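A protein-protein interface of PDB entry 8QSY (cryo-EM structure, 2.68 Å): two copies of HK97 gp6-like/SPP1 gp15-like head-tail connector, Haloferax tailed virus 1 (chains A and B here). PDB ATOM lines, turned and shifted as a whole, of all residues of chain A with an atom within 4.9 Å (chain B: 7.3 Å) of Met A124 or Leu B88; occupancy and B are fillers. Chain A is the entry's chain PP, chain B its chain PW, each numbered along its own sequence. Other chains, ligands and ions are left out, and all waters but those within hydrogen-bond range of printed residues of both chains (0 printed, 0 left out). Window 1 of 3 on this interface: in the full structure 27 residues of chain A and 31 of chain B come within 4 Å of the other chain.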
ATOM      1  N   TYR A  80      30.570  22.717  27.446  1.00  0.00           N
ATOM      2  CA  TYR A  80      29.340  22.123  27.957  1.00  0.00           C
ATOM      3  C   TYR A  80      28.564  23.094  28.843  1.00  0.00           C
ATOM      4  O   TYR A  80      27.346  23.141  28.773  1.00  0.00           O
ATOM      5  CB  TYR A  80      29.608  20.804  28.689  1.00  0.00           C
ATOM      6  CG  TYR A  80      29.997  19.668  27.777  1.00  0.00           C
ATOM      7  CD1 TYR A  80      29.238  19.361  26.652  1.00  0.00           C
ATOM      8  CD2 TYR A  80      31.125  18.894  28.037  1.00  0.00           C
ATOM      9  CE1 TYR A  80      29.614  18.345  25.788  1.00  0.00           C
ATOM     10  CE2 TYR A  80      31.507  17.871  27.181  1.00  0.00           C
ATOM     11  CZ  TYR A  80      30.741  17.588  26.062  1.00  0.00           C
ATOM     12  OH  TYR A  80      31.115  16.576  25.221  1.00  0.00           O
ATOM     13  N   ARG A 120      21.011  17.983  29.498  1.00  0.00           N
ATOM     14  CA  ARG A 120      22.000  16.964  29.161  1.00  0.00           C
ATOM     15  C   ARG A 120      23.428  17.517  29.137  1.00  0.00           C
ATOM     16  O   ARG A 120      24.351  16.866  29.626  1.00  0.00           O
ATOM     17  CB  ARG A 120      21.606  16.290  27.843  1.00  0.00           C
ATOM     18  CG  ARG A 120      21.664  17.177  26.608  1.00  0.00           C
ATOM     19  CD  ARG A 120      20.664  16.745  25.551  1.00  0.00           C
ATOM     20  NE  ARG A 120      20.820  17.513  24.330  1.00  0.00           N
ATOM     21  CZ  ARG A 120      20.038  18.502  23.895  1.00  0.00           C
ATOM     22  NH1 ARG A 120      20.325  19.089  22.749  1.00  0.00           N
ATOM     23  NH2 ARG A 120      18.978  18.907  24.560  1.00  0.00           N
ATOM     24  N   TYR A 121      23.602  18.736  28.628  1.00  0.00           N
ATOM     25  CA  TYR A 121      24.883  19.418  28.657  1.00  0.00           C
ATOM     26  C   TYR A 121      25.314  19.734  30.083  1.00  0.00           C
ATOM     27  O   TYR A 121      26.479  19.560  30.422  1.00  0.00           O
ATOM     28  CB  TYR A 121      24.794  20.686  27.820  1.00  0.00           C
ATOM     29  CG  TYR A 121      24.362  20.408  26.409  1.00  0.00           C
ATOM     30  CD1 TYR A 121      25.197  19.697  25.559  1.00  0.00           C
ATOM     31  CD2 TYR A 121      23.127  20.834  25.934  1.00  0.00           C
ATOM     32  CE1 TYR A 121      24.804  19.412  24.263  1.00  0.00           C
ATOM     33  CE2 TYR A 121      22.723  20.554  24.634  1.00  0.00           C
ATOM     34  CZ  TYR A 121      23.569  19.841  23.801  1.00  0.00           C
ATOM     35  OH  TYR A 121      23.208  19.555  22.518  1.00  0.00           O
ATOM     36  N   GLY A 122      24.367  20.155  30.926  1.00  0.00           N
ATOM     37  CA  GLY A 122      24.639  20.420  32.327  1.00  0.00           C
ATOM     38  C   GLY A 122      25.108  19.148  33.036  1.00  0.00           C
ATOM     39  O   GLY A 122      26.121  19.168  33.716  1.00  0.00           O
ATOM     40  N   ARG A 123      24.428  18.021  32.802  1.00  0.00           N
ATOM     41  CA  ARG A 123      24.792  16.731  33.374  1.00  0.00           C
ATOM     42  C   ARG A 123      26.168  16.253  32.909  1.00  0.00           C
ATOM     43  O   ARG A 123      26.901  15.670  33.698  1.00  0.00           O
ATOM     44  CB  ARG A 123      23.717  15.692  33.067  1.00  0.00           C
ATOM     45  CG  ARG A 123      22.418  15.975  33.800  1.00  0.00           C
ATOM     46  CD  ARG A 123      21.379  14.903  33.576  1.00  0.00           C
ATOM     47  NE  ARG A 123      20.832  14.748  32.235  1.00  0.00           N
ATOM     48  CZ  ARG A 123      19.681  15.236  31.786  1.00  0.00           C
ATOM     49  NH1 ARG A 123      19.276  14.923  30.569  1.00  0.00           N
ATOM     50  NH2 ARG A 123      18.938  16.027  32.532  1.00  0.00           N
ATOM     51  N   MET A 124      26.547  16.534  31.659  1.00  0.00           N
ATOM     52  CA  MET A 124      27.905  16.287  31.205  1.00  0.00           C
ATOM     53  C   MET A 124      28.912  17.169  31.939  1.00  0.00           C
ATOM     54  O   MET A 124      29.838  16.643  32.532  1.00  0.00           O
ATOM     55  CB  MET A 124      28.028  16.452  29.694  1.00  0.00           C
ATOM     56  CG  MET A 124      27.440  15.265  28.988  1.00  0.00           C
ATOM     57  SD  MET A 124      27.880  15.144  27.251  1.00  0.00           S
ATOM     58  CE  MET A 124      26.839  16.425  26.555  1.00  0.00           C
ATOM     59  N   ALA A 125      28.706  18.491  31.959  1.00  0.00           N
ATOM     60  CA  ALA A 125      29.579  19.426  32.658  1.00  0.00           C
ATOM     61  C   ALA A 125      29.783  19.016  34.119  1.00  0.00           C
ATOM     62  O   ALA A 125      30.887  19.075  34.641  1.00  0.00           O
ATOM     63  CB  ALA A 125      28.992  20.812  32.545  1.00  0.00           C
ATOM     64  N   LEU A 126      28.728  18.525  34.763  1.00  0.00           N
ATOM     65  CA  LEU A 126      28.712  18.144  36.167  1.00  0.00           C
ATOM     66  C   LEU A 126      29.748  17.059  36.502  1.00  0.00           C
ATOM     67  O   LEU A 126      30.361  17.117  37.564  1.00  0.00           O
ATOM     68  CB  LEU A 126      27.269  17.736  36.475  1.00  0.00           C
ATOM     69  CG  LEU A 126      26.817  17.719  37.936  1.00  0.00           C
ATOM     70  CD1 LEU A 126      27.178  18.993  38.698  1.00  0.00           C
ATOM     71  CD2 LEU A 126      25.305  17.535  37.978  1.00  0.00           C
ATOM     72  N   GLU A 127      30.039  16.119  35.592  1.00  0.00           N
ATOM     73  CA  GLU A 127      31.065  15.101  35.805  1.00  0.00           C
ATOM     74  C   GLU A 127      32.492  15.671  35.820  1.00  0.00           C
ATOM     75  O   GLU A 127      33.386  15.051  36.384  1.00  0.00           O
ATOM     76  CB  GLU A 127      30.952  13.992  34.753  1.00  0.00           C
ATOM     77  CG  GLU A 127      29.802  13.012  34.979  1.00  0.00           C
ATOM     78  CD  GLU A 127      30.046  11.800  35.879  1.00  0.00           C
ATOM     79  OE1 GLU A 127      31.192  11.579  36.335  1.00  0.00           O
ATOM     80  OE2 GLU A 127      29.084  11.052  36.172  1.00  0.00           O
ATOM     81  N   TYR A 128      32.725  16.852  35.235  1.00  0.00           N
ATOM     82  CA  TYR A 128      34.045  17.474  35.206  1.00  0.00           C
ATOM     83  C   TYR A 128      34.418  18.134  36.536  1.00  0.00           C
ATOM     84  O   TYR A 128      35.587  18.452  36.755  1.00  0.00           O
ATOM     85  CB  TYR A 128      34.117  18.522  34.092  1.00  0.00           C
ATOM     86  CG  TYR A 128      34.177  17.957  32.692  1.00  0.00           C
ATOM     87  CD1 TYR A 128      33.101  17.254  32.152  1.00  0.00           C
ATOM     88  CD2 TYR A 128      35.301  18.157  31.893  1.00  0.00           C
ATOM     89  CE1 TYR A 128      33.165  16.725  30.866  1.00  0.00           C
ATOM     90  CE2 TYR A 128      35.377  17.628  30.610  1.00  0.00           C
ATOM     91  CZ  TYR A 128      34.307  16.906  30.100  1.00  0.00           C
ATOM     92  OH  TYR A 128      34.387  16.356  28.852  1.00  0.00           O
ATOM     93  N   TRP B  37      23.627   8.143  12.558  1.00  0.00           N
ATOM     94  CA  TRP B  37      23.423   9.578  12.759  1.00  0.00           C
ATOM     95  C   TRP B  37      23.746  10.385  11.490  1.00  0.00           C
ATOM     96  O   TRP B  37      24.444  11.399  11.559  1.00  0.00           O
ATOM     97  CB  TRP B  37      24.214  10.090  13.979  1.00  0.00           C
ATOM     98  CG  TRP B  37      24.073   9.298  15.244  1.00  0.00           C
ATOM     99  CD1 TRP B  37      23.042   9.356  16.136  1.00  0.00           C
ATOM    100  CD2 TRP B  37      25.016   8.345  15.789  1.00  0.00           C
ATOM    101  NE1 TRP B  37      23.279   8.500  17.182  1.00  0.00           N
ATOM    102  CE2 TRP B  37      24.491   7.870  17.015  1.00  0.00           C
ATOM    103  CE3 TRP B  37      26.258   7.851  15.372  1.00  0.00           C
ATOM    104  CZ2 TRP B  37      25.162   6.915  17.801  1.00  0.00           C
ATOM    105  CZ3 TRP B  37      26.929   6.919  16.147  1.00  0.00           C
ATOM    106  CH2 TRP B  37      26.386   6.457  17.350  1.00  0.00           C
ATOM    107  N   SER B  51      35.995  15.226  22.209  1.00  0.00           N
ATOM    108  CA  SER B  51      35.527  15.343  23.578  1.00  0.00           C
ATOM    109  C   SER B  51      35.613  14.017  24.339  1.00  0.00           C
ATOM    110  O   SER B  51      36.052  14.010  25.481  1.00  0.00           O
ATOM    111  CB  SER B  51      34.150  15.913  23.611  1.00  0.00           C
ATOM    112  OG  SER B  51      33.762  16.168  24.948  1.00  0.00           O
ATOM    113  N   GLU B  55      37.892  13.450  27.568  1.00  0.00           N
ATOM    114  CA  GLU B  55      37.192  13.044  28.771  1.00  0.00           C
ATOM    115  C   GLU B  55      37.729  11.715  29.303  1.00  0.00           C
ATOM    116  O   GLU B  55      37.894  11.581  30.508  1.00  0.00           O
ATOM    117  CB  GLU B  55      35.707  12.974  28.456  1.00  0.00           C
ATOM    118  CG  GLU B  55      34.861  12.776  29.676  1.00  0.00           C
ATOM    119  CD  GLU B  55      33.392  13.005  29.374  1.00  0.00           C
ATOM    120  OE1 GLU B  55      33.029  14.134  28.981  1.00  0.00           O
ATOM    121  OE2 GLU B  55      32.604  12.047  29.489  1.00  0.00           O
ATOM    122  N   LEU B  59      38.961  12.234  33.008  1.00  0.00           N
ATOM    123  CA  LEU B  59      38.002  11.764  34.008  1.00  0.00           C
ATOM    124  C   LEU B  59      38.052  10.253  34.252  1.00  0.00           C
ATOM    125  O   LEU B  59      37.636   9.797  35.316  1.00  0.00           O
ATOM    126  CB  LEU B  59      36.582  12.163  33.601  1.00  0.00           C
ATOM    127  CG  LEU B  59      36.308  13.660  33.550  1.00  0.00           C
ATOM    128  CD1 LEU B  59      34.835  13.915  33.300  1.00  0.00           C
ATOM    129  CD2 LEU B  59      36.727  14.317  34.856  1.00  0.00           C
ATOM    130  N   LEU B  81      31.763   6.025  24.570  1.00  0.00           N
ATOM    131  CA  LEU B  81      31.751   7.382  25.083  1.00  0.00           C
ATOM    132  C   LEU B  81      31.499   8.407  23.970  1.00  0.00           C
ATOM    133  O   LEU B  81      30.784   9.381  24.185  1.00  0.00           O
ATOM    134  CB  LEU B  81      33.071   7.602  25.818  1.00  0.00           C
ATOM    135  CG  LEU B  81      33.120   8.842  26.698  1.00  0.00           C
ATOM    136  CD1 LEU B  81      32.157   8.698  27.869  1.00  0.00           C
ATOM    137  CD2 LEU B  81      34.532   9.029  27.233  1.00  0.00           C
ATOM    138  N   SER B  82      32.017   8.157  22.762  1.00  0.00           N
ATOM    139  CA  SER B  82      31.766   8.974  21.579  1.00  0.00           C
ATOM    140  C   SER B  82      30.303   8.888  21.142  1.00  0.00           C
ATOM    141  O   SER B  82      29.661   9.914  20.952  1.00  0.00           O
ATOM    142  CB  SER B  82      32.675   8.601  20.439  1.00  0.00           C
ATOM    143  OG  SER B  82      34.029   8.640  20.840  1.00  0.00           O
ATOM    144  N   ALA B  83      29.755   7.674  21.016  1.00  0.00           N
ATOM    145  CA  ALA B  83      28.361   7.444  20.656  1.00  0.00           C
ATOM    146  C   ALA B  83      27.401   8.069  21.678  1.00  0.00           C
ATOM    147  O   ALA B  83      26.389   8.649  21.295  1.00  0.00           O
ATOM    148  CB  ALA B  83      28.131   5.964  20.486  1.00  0.00           C
ATOM    149  N   HIS B  84      27.744   8.014  22.972  1.00  0.00           N
ATOM    150  CA  HIS B  84      26.999   8.691  24.024  1.00  0.00           C
ATOM    151  C   HIS B  84      26.893  10.186  23.735  1.00  0.00           C
ATOM    152  O   HIS B  84      25.789  10.714  23.698  1.00  0.00           O
ATOM    153  CB  HIS B  84      27.610   8.395  25.395  1.00  0.00           C
ATOM    154  CG  HIS B  84      27.007   9.180  26.517  1.00  0.00           C
ATOM    155  ND1 HIS B  84      25.713   9.018  27.018  1.00  0.00           N
ATOM    156  CD2 HIS B  84      27.540  10.204  27.210  1.00  0.00           C
ATOM    157  CE1 HIS B  84      25.518   9.897  27.997  1.00  0.00           C
ATOM    158  NE2 HIS B  84      26.619  10.622  28.127  1.00  0.00           N
ATOM    159  N   LYS B  85      28.023  10.848  23.457  1.00  0.00           N
ATOM    160  CA  LYS B  85      28.048  12.260  23.115  1.00  0.00           C
ATOM    161  C   LYS B  85      27.261  12.561  21.844  1.00  0.00           C
ATOM    162  O   LYS B  85      26.410  13.439  21.885  1.00  0.00           O
ATOM    163  CB  LYS B  85      29.481  12.776  23.099  1.00  0.00           C
ATOM    164  CG  LYS B  85      29.955  13.112  24.500  1.00  0.00           C
ATOM    165  CD  LYS B  85      31.423  12.906  24.756  1.00  0.00           C
ATOM    166  CE  LYS B  85      31.919  13.520  26.051  1.00  0.00           C
ATOM    167  NZ  LYS B  85      31.108  13.182  27.245  1.00  0.00           N
ATOM    168  N   ILE B  86      27.454  11.815  20.745  1.00  0.00           N
ATOM    169  CA  ILE B  86      26.700  12.070  19.517  1.00  0.00           C
ATOM    170  C   ILE B  86      25.194  11.989  19.770  1.00  0.00           C
ATOM    171  O   ILE B  86      24.448  12.865  19.337  1.00  0.00           O
ATOM    172  CB  ILE B  86      27.125  11.145  18.359  1.00  0.00           C
ATOM    173  CG1 ILE B  86      28.590  11.345  17.977  1.00  0.00           C
ATOM    174  CG2 ILE B  86      26.237  11.363  17.139  1.00  0.00           C
ATOM    175  CD1 ILE B  86      29.183  10.176  17.229  1.00  0.00           C
ATOM    176  N   GLN B  87      24.746  10.974  20.514  1.00  0.00           N
ATOM    177  CA  GLN B  87      23.340  10.798  20.844  1.00  0.00           C
ATOM    178  C   GLN B  87      22.788  11.946  21.698  1.00  0.00           C
ATOM    179  O   GLN B  87      21.641  12.339  21.522  1.00  0.00           O
ATOM    180  CB  GLN B  87      23.137   9.446  21.521  1.00  0.00           C
ATOM    181  CG  GLN B  87      21.668   9.065  21.665  1.00  0.00           C
ATOM    182  CD  GLN B  87      21.002   8.830  20.329  1.00  0.00           C
ATOM    183  OE1 GLN B  87      21.509   8.087  19.493  1.00  0.00           O
ATOM    184  NE2 GLN B  87      19.859   9.451  20.098  1.00  0.00           N
ATOM    185  N   LEU B  88      23.586  12.526  22.602  1.00  0.00           N
ATOM    186  CA  LEU B  88      23.178  13.728  23.318  1.00  0.00           C
ATOM    187  C   LEU B  88      23.190  14.980  22.439  1.00  0.00           C
ATOM    188  O   LEU B  88      22.350  15.850  22.650  1.00  0.00           O
ATOM    189  CB  LEU B  88      24.039  13.923  24.564  1.00  0.00           C
ATOM    190  CG  LEU B  88      23.887  12.865  25.654  1.00  0.00           C
ATOM    191  CD1 LEU B  88      24.680  13.291  26.865  1.00  0.00           C
ATOM    192  CD2 LEU B  88      22.429  12.677  26.036  1.00  0.00           C
ATOM    193  N   PHE B  89      24.073  15.074  21.435  1.00  0.00           N
ATOM    194  CA  PHE B  89      24.036  16.182  20.485  1.00  0.00           C
ATOM    195  C   PHE B  89      22.785  16.099  19.597  1.00  0.00           C
ATOM    196  O   PHE B  89      22.266  17.131  19.172  1.00  0.00           O
ATOM    197  CB  PHE B  89      25.316  16.234  19.644  1.00  0.00           C
ATOM    198  CG  PHE B  89      26.647  16.427  20.340  1.00  0.00           C
ATOM    199  CD1 PHE B  89      26.774  16.496  21.727  1.00  0.00           C
ATOM    200  CD2 PHE B  89      27.809  16.519  19.581  1.00  0.00           C
ATOM    201  CE1 PHE B  89      28.025  16.636  22.326  1.00  0.00           C
ATOM    202  CE2 PHE B  89      29.055  16.675  20.177  1.00  0.00           C
ATOM    203  CZ  PHE B  89      29.161  16.723  21.548  1.00  0.00           C
ATOM    204  N   GLU B  90      22.270  14.884  19.369  1.00  0.00           N
ATOM    205  CA  GLU B  90      20.996  14.621  18.703  1.00  0.00           C
ATOM    206  C   GLU B  90      19.767  14.889  19.589  1.00  0.00           C
ATOM    207  O   GLU B  90      18.635  14.723  19.124  1.00  0.00           O
ATOM    208  CB  GLU B  90      20.991  13.176  18.199  1.00  0.00           C
ATOM    209  CG  GLU B  90      21.903  12.944  17.011  1.00  0.00           C
ATOM    210  CD  GLU B  90      21.169  12.640  15.714  1.00  0.00           C
ATOM    211  OE1 GLU B  90      20.224  11.818  15.751  1.00  0.00           O
ATOM    212  OE2 GLU B  90      21.556  13.198  14.653  1.00  0.00           O
ATOM    213  N   GLY B  91      19.953  15.282  20.858  1.00  0.00           N
ATOM    214  CA  GLY B  91      18.856  15.658  21.742  1.00  0.00           C
ATOM    215  C   GLY B  91      18.509  14.631  22.826  1.00  0.00           C
ATOM    216  O   GLY B  91      17.627  14.896  23.644  1.00  0.00           O
ATOM    217  N   GLY B  92      19.194  13.477  22.857  1.00  0.00           N
ATOM    218  CA  GLY B  92      18.969  12.443  23.862  1.00  0.00           C
ATOM    219  C   GLY B  92      18.494  11.121  23.259  1.00  0.00           C
ATOM    220  O   GLY B  92      18.405  10.976  22.039  1.00  0.00           O
ATOM    221  N   GLU B  93      18.209  10.141  24.126  1.00  0.00           N
ATOM    222  CA  GLU B  93      17.504   8.931  23.730  1.00  0.00           C
ATOM    223  C   GLU B  93      16.074   9.278  23.323  1.00  0.00           C
ATOM    224  O   GLU B  93      15.346   9.890  24.100  1.00  0.00           O
ATOM    225  CB  GLU B  93      17.348   8.003  24.936  1.00  0.00           C
ATOM    226  CG  GLU B  93      18.586   7.225  25.311  1.00  0.00           C
ATOM    227  CD  GLU B  93      18.941   6.083  24.386  1.00  0.00           C
ATOM    228  OE1 GLU B  93      18.138   5.741  23.493  1.00  0.00           O
ATOM    229  OE2 GLU B  93      20.042   5.533  24.551  1.00  0.00           O
ATOM    230  N   LYS B 114      22.354  10.414  36.365  1.00  0.00           N
ATOM    231  CA  LYS B 114      23.704  10.885  36.063  1.00  0.00           C
ATOM    232  C   LYS B 114      24.035  10.720  34.581  1.00  0.00           C
ATOM    233  O   LYS B 114      23.471   9.865  33.913  1.00  0.00           O
ATOM    234  CB  LYS B 114      24.712  10.165  36.959  1.00  0.00           C
ATOM    235  CG  LYS B 114      24.533  10.503  38.432  1.00  0.00           C
ATOM    236  CD  LYS B 114      25.464   9.762  39.363  1.00  0.00           C
ATOM    237  CE  LYS B 114      25.535  10.361  40.756  1.00  0.00           C
ATOM    238  NZ  LYS B 114      24.272  10.193  41.514  1.00  0.00           N
ATOM    239  N   ASP B 115      25.005  11.496  34.088  1.00  0.00           N
ATOM    240  CA  ASP B 115      25.387  11.587  32.683  1.00  0.00           C
ATOM    241  C   ASP B 115      25.357  10.252  31.917  1.00  0.00           C
ATOM    242  O   ASP B 115      24.528  10.061  31.020  1.00  0.00           O
ATOM    243  CB  ASP B 115      26.748  12.272  32.591  1.00  0.00           C
ATOM    244  CG  ASP B 115      27.320  12.336  31.187  1.00  0.00           C
ATOM    245  OD1 ASP B 115      26.526  12.342  30.235  1.00  0.00           O
ATOM    246  OD2 ASP B 115      28.560  12.378  31.055  1.00  0.00           O
ATOM    247  N   LEU B 116      26.243   9.308  32.264  1.00  0.00           N
ATOM    248  CA  LEU B 116      26.360   8.072  31.502  1.00  0.00           C
ATOM    249  C   LEU B 116      25.106   7.196  31.595  1.00  0.00           C
ATOM    250  O   LEU B 116      24.815   6.460  30.671  1.00  0.00           O
ATOM    251  CB  LEU B 116      27.632   7.311  31.889  1.00  0.00           C
ATOM    252  CG  LEU B 116      28.960   7.987  31.536  1.00  0.00           C
ATOM    253  CD1 LEU B 116      30.129   7.093  31.897  1.00  0.00           C
ATOM    254  CD2 LEU B 116      29.050   8.332  30.060  1.00  0.00           C
ATOM    255  N   LYS B 118      22.123   8.083  31.212  1.00  0.00           N
ATOM    256  CA  LYS B 118      21.035   8.687  30.447  1.00  0.00           C
ATOM    257  C   LYS B 118      20.907   8.184  29.004  1.00  0.00           C
ATOM    258  O   LYS B 118      19.914   8.504  28.355  1.00  0.00           O
ATOM    259  CB  LYS B 118      21.110  10.216  30.512  1.00  0.00           C
ATOM    260  CG  LYS B 118      20.940  10.805  31.910  1.00  0.00           C
ATOM    261  CD  LYS B 118      19.541  11.325  32.262  1.00  0.00           C
ATOM    262  CE  LYS B 118      18.389  10.359  32.058  1.00  0.00           C
ATOM    263  NZ  LYS B 118      17.280  10.600  33.015  1.00  0.00           N
ATOM    264  N   THR B 119      21.874   7.402  28.492  1.00  0.00           N
ATOM    265  CA  THR B 119      21.720   6.736  27.195  1.00  0.00           C
ATOM    266  C   THR B 119      22.312   5.321  27.212  1.00  0.00           C
ATOM    267  O   THR B 119      23.157   5.017  28.037  1.00  0.00           O
ATOM    268  CB  THR B 119      22.236   7.564  26.001  1.00  0.00           C
ATOM    269  OG1 THR B 119      23.610   7.327  25.721  1.00  0.00           O
ATOM    270  CG2 THR B 119      22.072   9.063  26.115  1.00  0.00           C
ATOM    271  N   TYR B 121      24.446   3.847  25.128  1.00  0.00           N
ATOM    272  CA  TYR B 121      25.885   3.889  24.935  1.00  0.00           C
ATOM    273  C   TYR B 121      26.618   4.273  26.214  1.00  0.00           C
ATOM    274  O   TYR B 121      27.667   3.714  26.512  1.00  0.00           O
ATOM    275  CB  TYR B 121      26.222   4.856  23.807  1.00  0.00           C
ATOM    276  CG  TYR B 121      25.504   4.536  22.527  1.00  0.00           C
ATOM    277  CD1 TYR B 121      25.764   3.343  21.867  1.00  0.00           C
ATOM    278  CD2 TYR B 121      24.561   5.399  21.984  1.00  0.00           C
ATOM    279  CE1 TYR B 121      25.100   3.003  20.701  1.00  0.00           C
ATOM    280  CE2 TYR B 121      23.883   5.071  20.815  1.00  0.00           C
ATOM    281  CZ  TYR B 121      24.158   3.872  20.176  1.00  0.00           C
ATOM    282  OH  TYR B 121      23.504   3.529  19.032  1.00  0.00           O
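Among the printed residues, pairs that only touch across the chains: Tyr A80 with Lys B85 (3.3 Å), Met A124 with Asp B115 (3.3 Å), Arg A123 with Asp B115 (3.6 Å), Glu A127 with Leu B59 (3.6 Å), Arg A123 with Lys B118 (3.7 Å), Met A124 with Leu B88 (3.7 Å), Arg A120 with Gly B91 (3.7 Å), Tyr A121 with Leu B88 (3.8 Å), Tyr A128 with Leu B59 (3.9 Å), Glu A127 with Asp B115 (3.9 Å) and Tyr A128 with Ser B51 (3.96 Å).
Of chain B, only Lys B85 (3.8 Å), Leu B88 (3.7 Å) and Asp B115 (3.3 Å) come within 4 Å of Met A124. Leu B88 touches just these residues of chain A: Arg A120 (2.8 Å), Tyr A121 (3.8 Å) and Met A124 (3.7 Å). Of the printed residues of chain A, Leu B59 touches Glu A127 and Tyr A128. Printed residues of chain B within 4 Å of Glu A127: Leu B59 and Asp B115. Of the printed residues of chain B, Arg A120 touches Leu B88 (2.8 Å) and Gly B91 (3.7 Å). Printed residues of chain A within 4 Å of Lys B85: Tyr A80 (3.3 Å) and Met A124 (3.8 Å). The nearest residue of chain B that does not touch Met A124 is Phe B89 (4.4 Å).
The side-chain hydroxyl (OG) of Ser B51 lies within hydrogen-bond range of the side-chain hydroxyl (OH) of Tyr A80 (2.7 Å). NE of Arg A120 sits at hydrogen-bond distance from O of Leu B88, at 2.8 Å. The side-chain sulfur (SD) of Met A124 lies within hydrogen-bond range of the side-chain amino group (NZ) of Lys B85, 3.8 Å away. OH of Tyr A128 sits at hydrogen-bond distance from OE1 of Glu B55 (2.6 Å).
The side-chain hydroxyl (OH) of Tyr A121 sits at hydrogen-bond distance from the guanidinium group (NH1) of Arg A120, at 2.9 Å. The side-chain carboxylate (OE1) of Glu B55 lies within salt-bridge range of the side-chain amino group (NZ) of Lys B85, 2.8 Å away. The side-chain carboxylate of Asp B115 is in hydrogen-bond range of a ring nitrogen (NE2) of His B84, at 2.7 Å.
1 position is printed for both chains. Of the 15 pairs that touch across the chains among the printed residues, none has its exchanged pair printed and touching as well.
Of the 23 printed residues of chain B, 8 touch a printed residue of chain A. Hydrophobic or aromatic side chains of chain B within 4 Å of the printed part of chain A: Leu B59 and Leu B88. Of the 10 printed residues of chain A, 7 touch a printed residue of chain B. Printed residues of chain A that touch a printed residue of chain B: Tyr A80, Arg A120, Tyr A121, Arg A123, Met A124, Glu A127 and Tyr A128. Hydrophobic or aromatic side chains of chain A that line the printed part of chain B: Tyr A80, Tyr A121, Met A124 and Tyr A128. Among the printed residues, 15 pairs touch across the chains.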
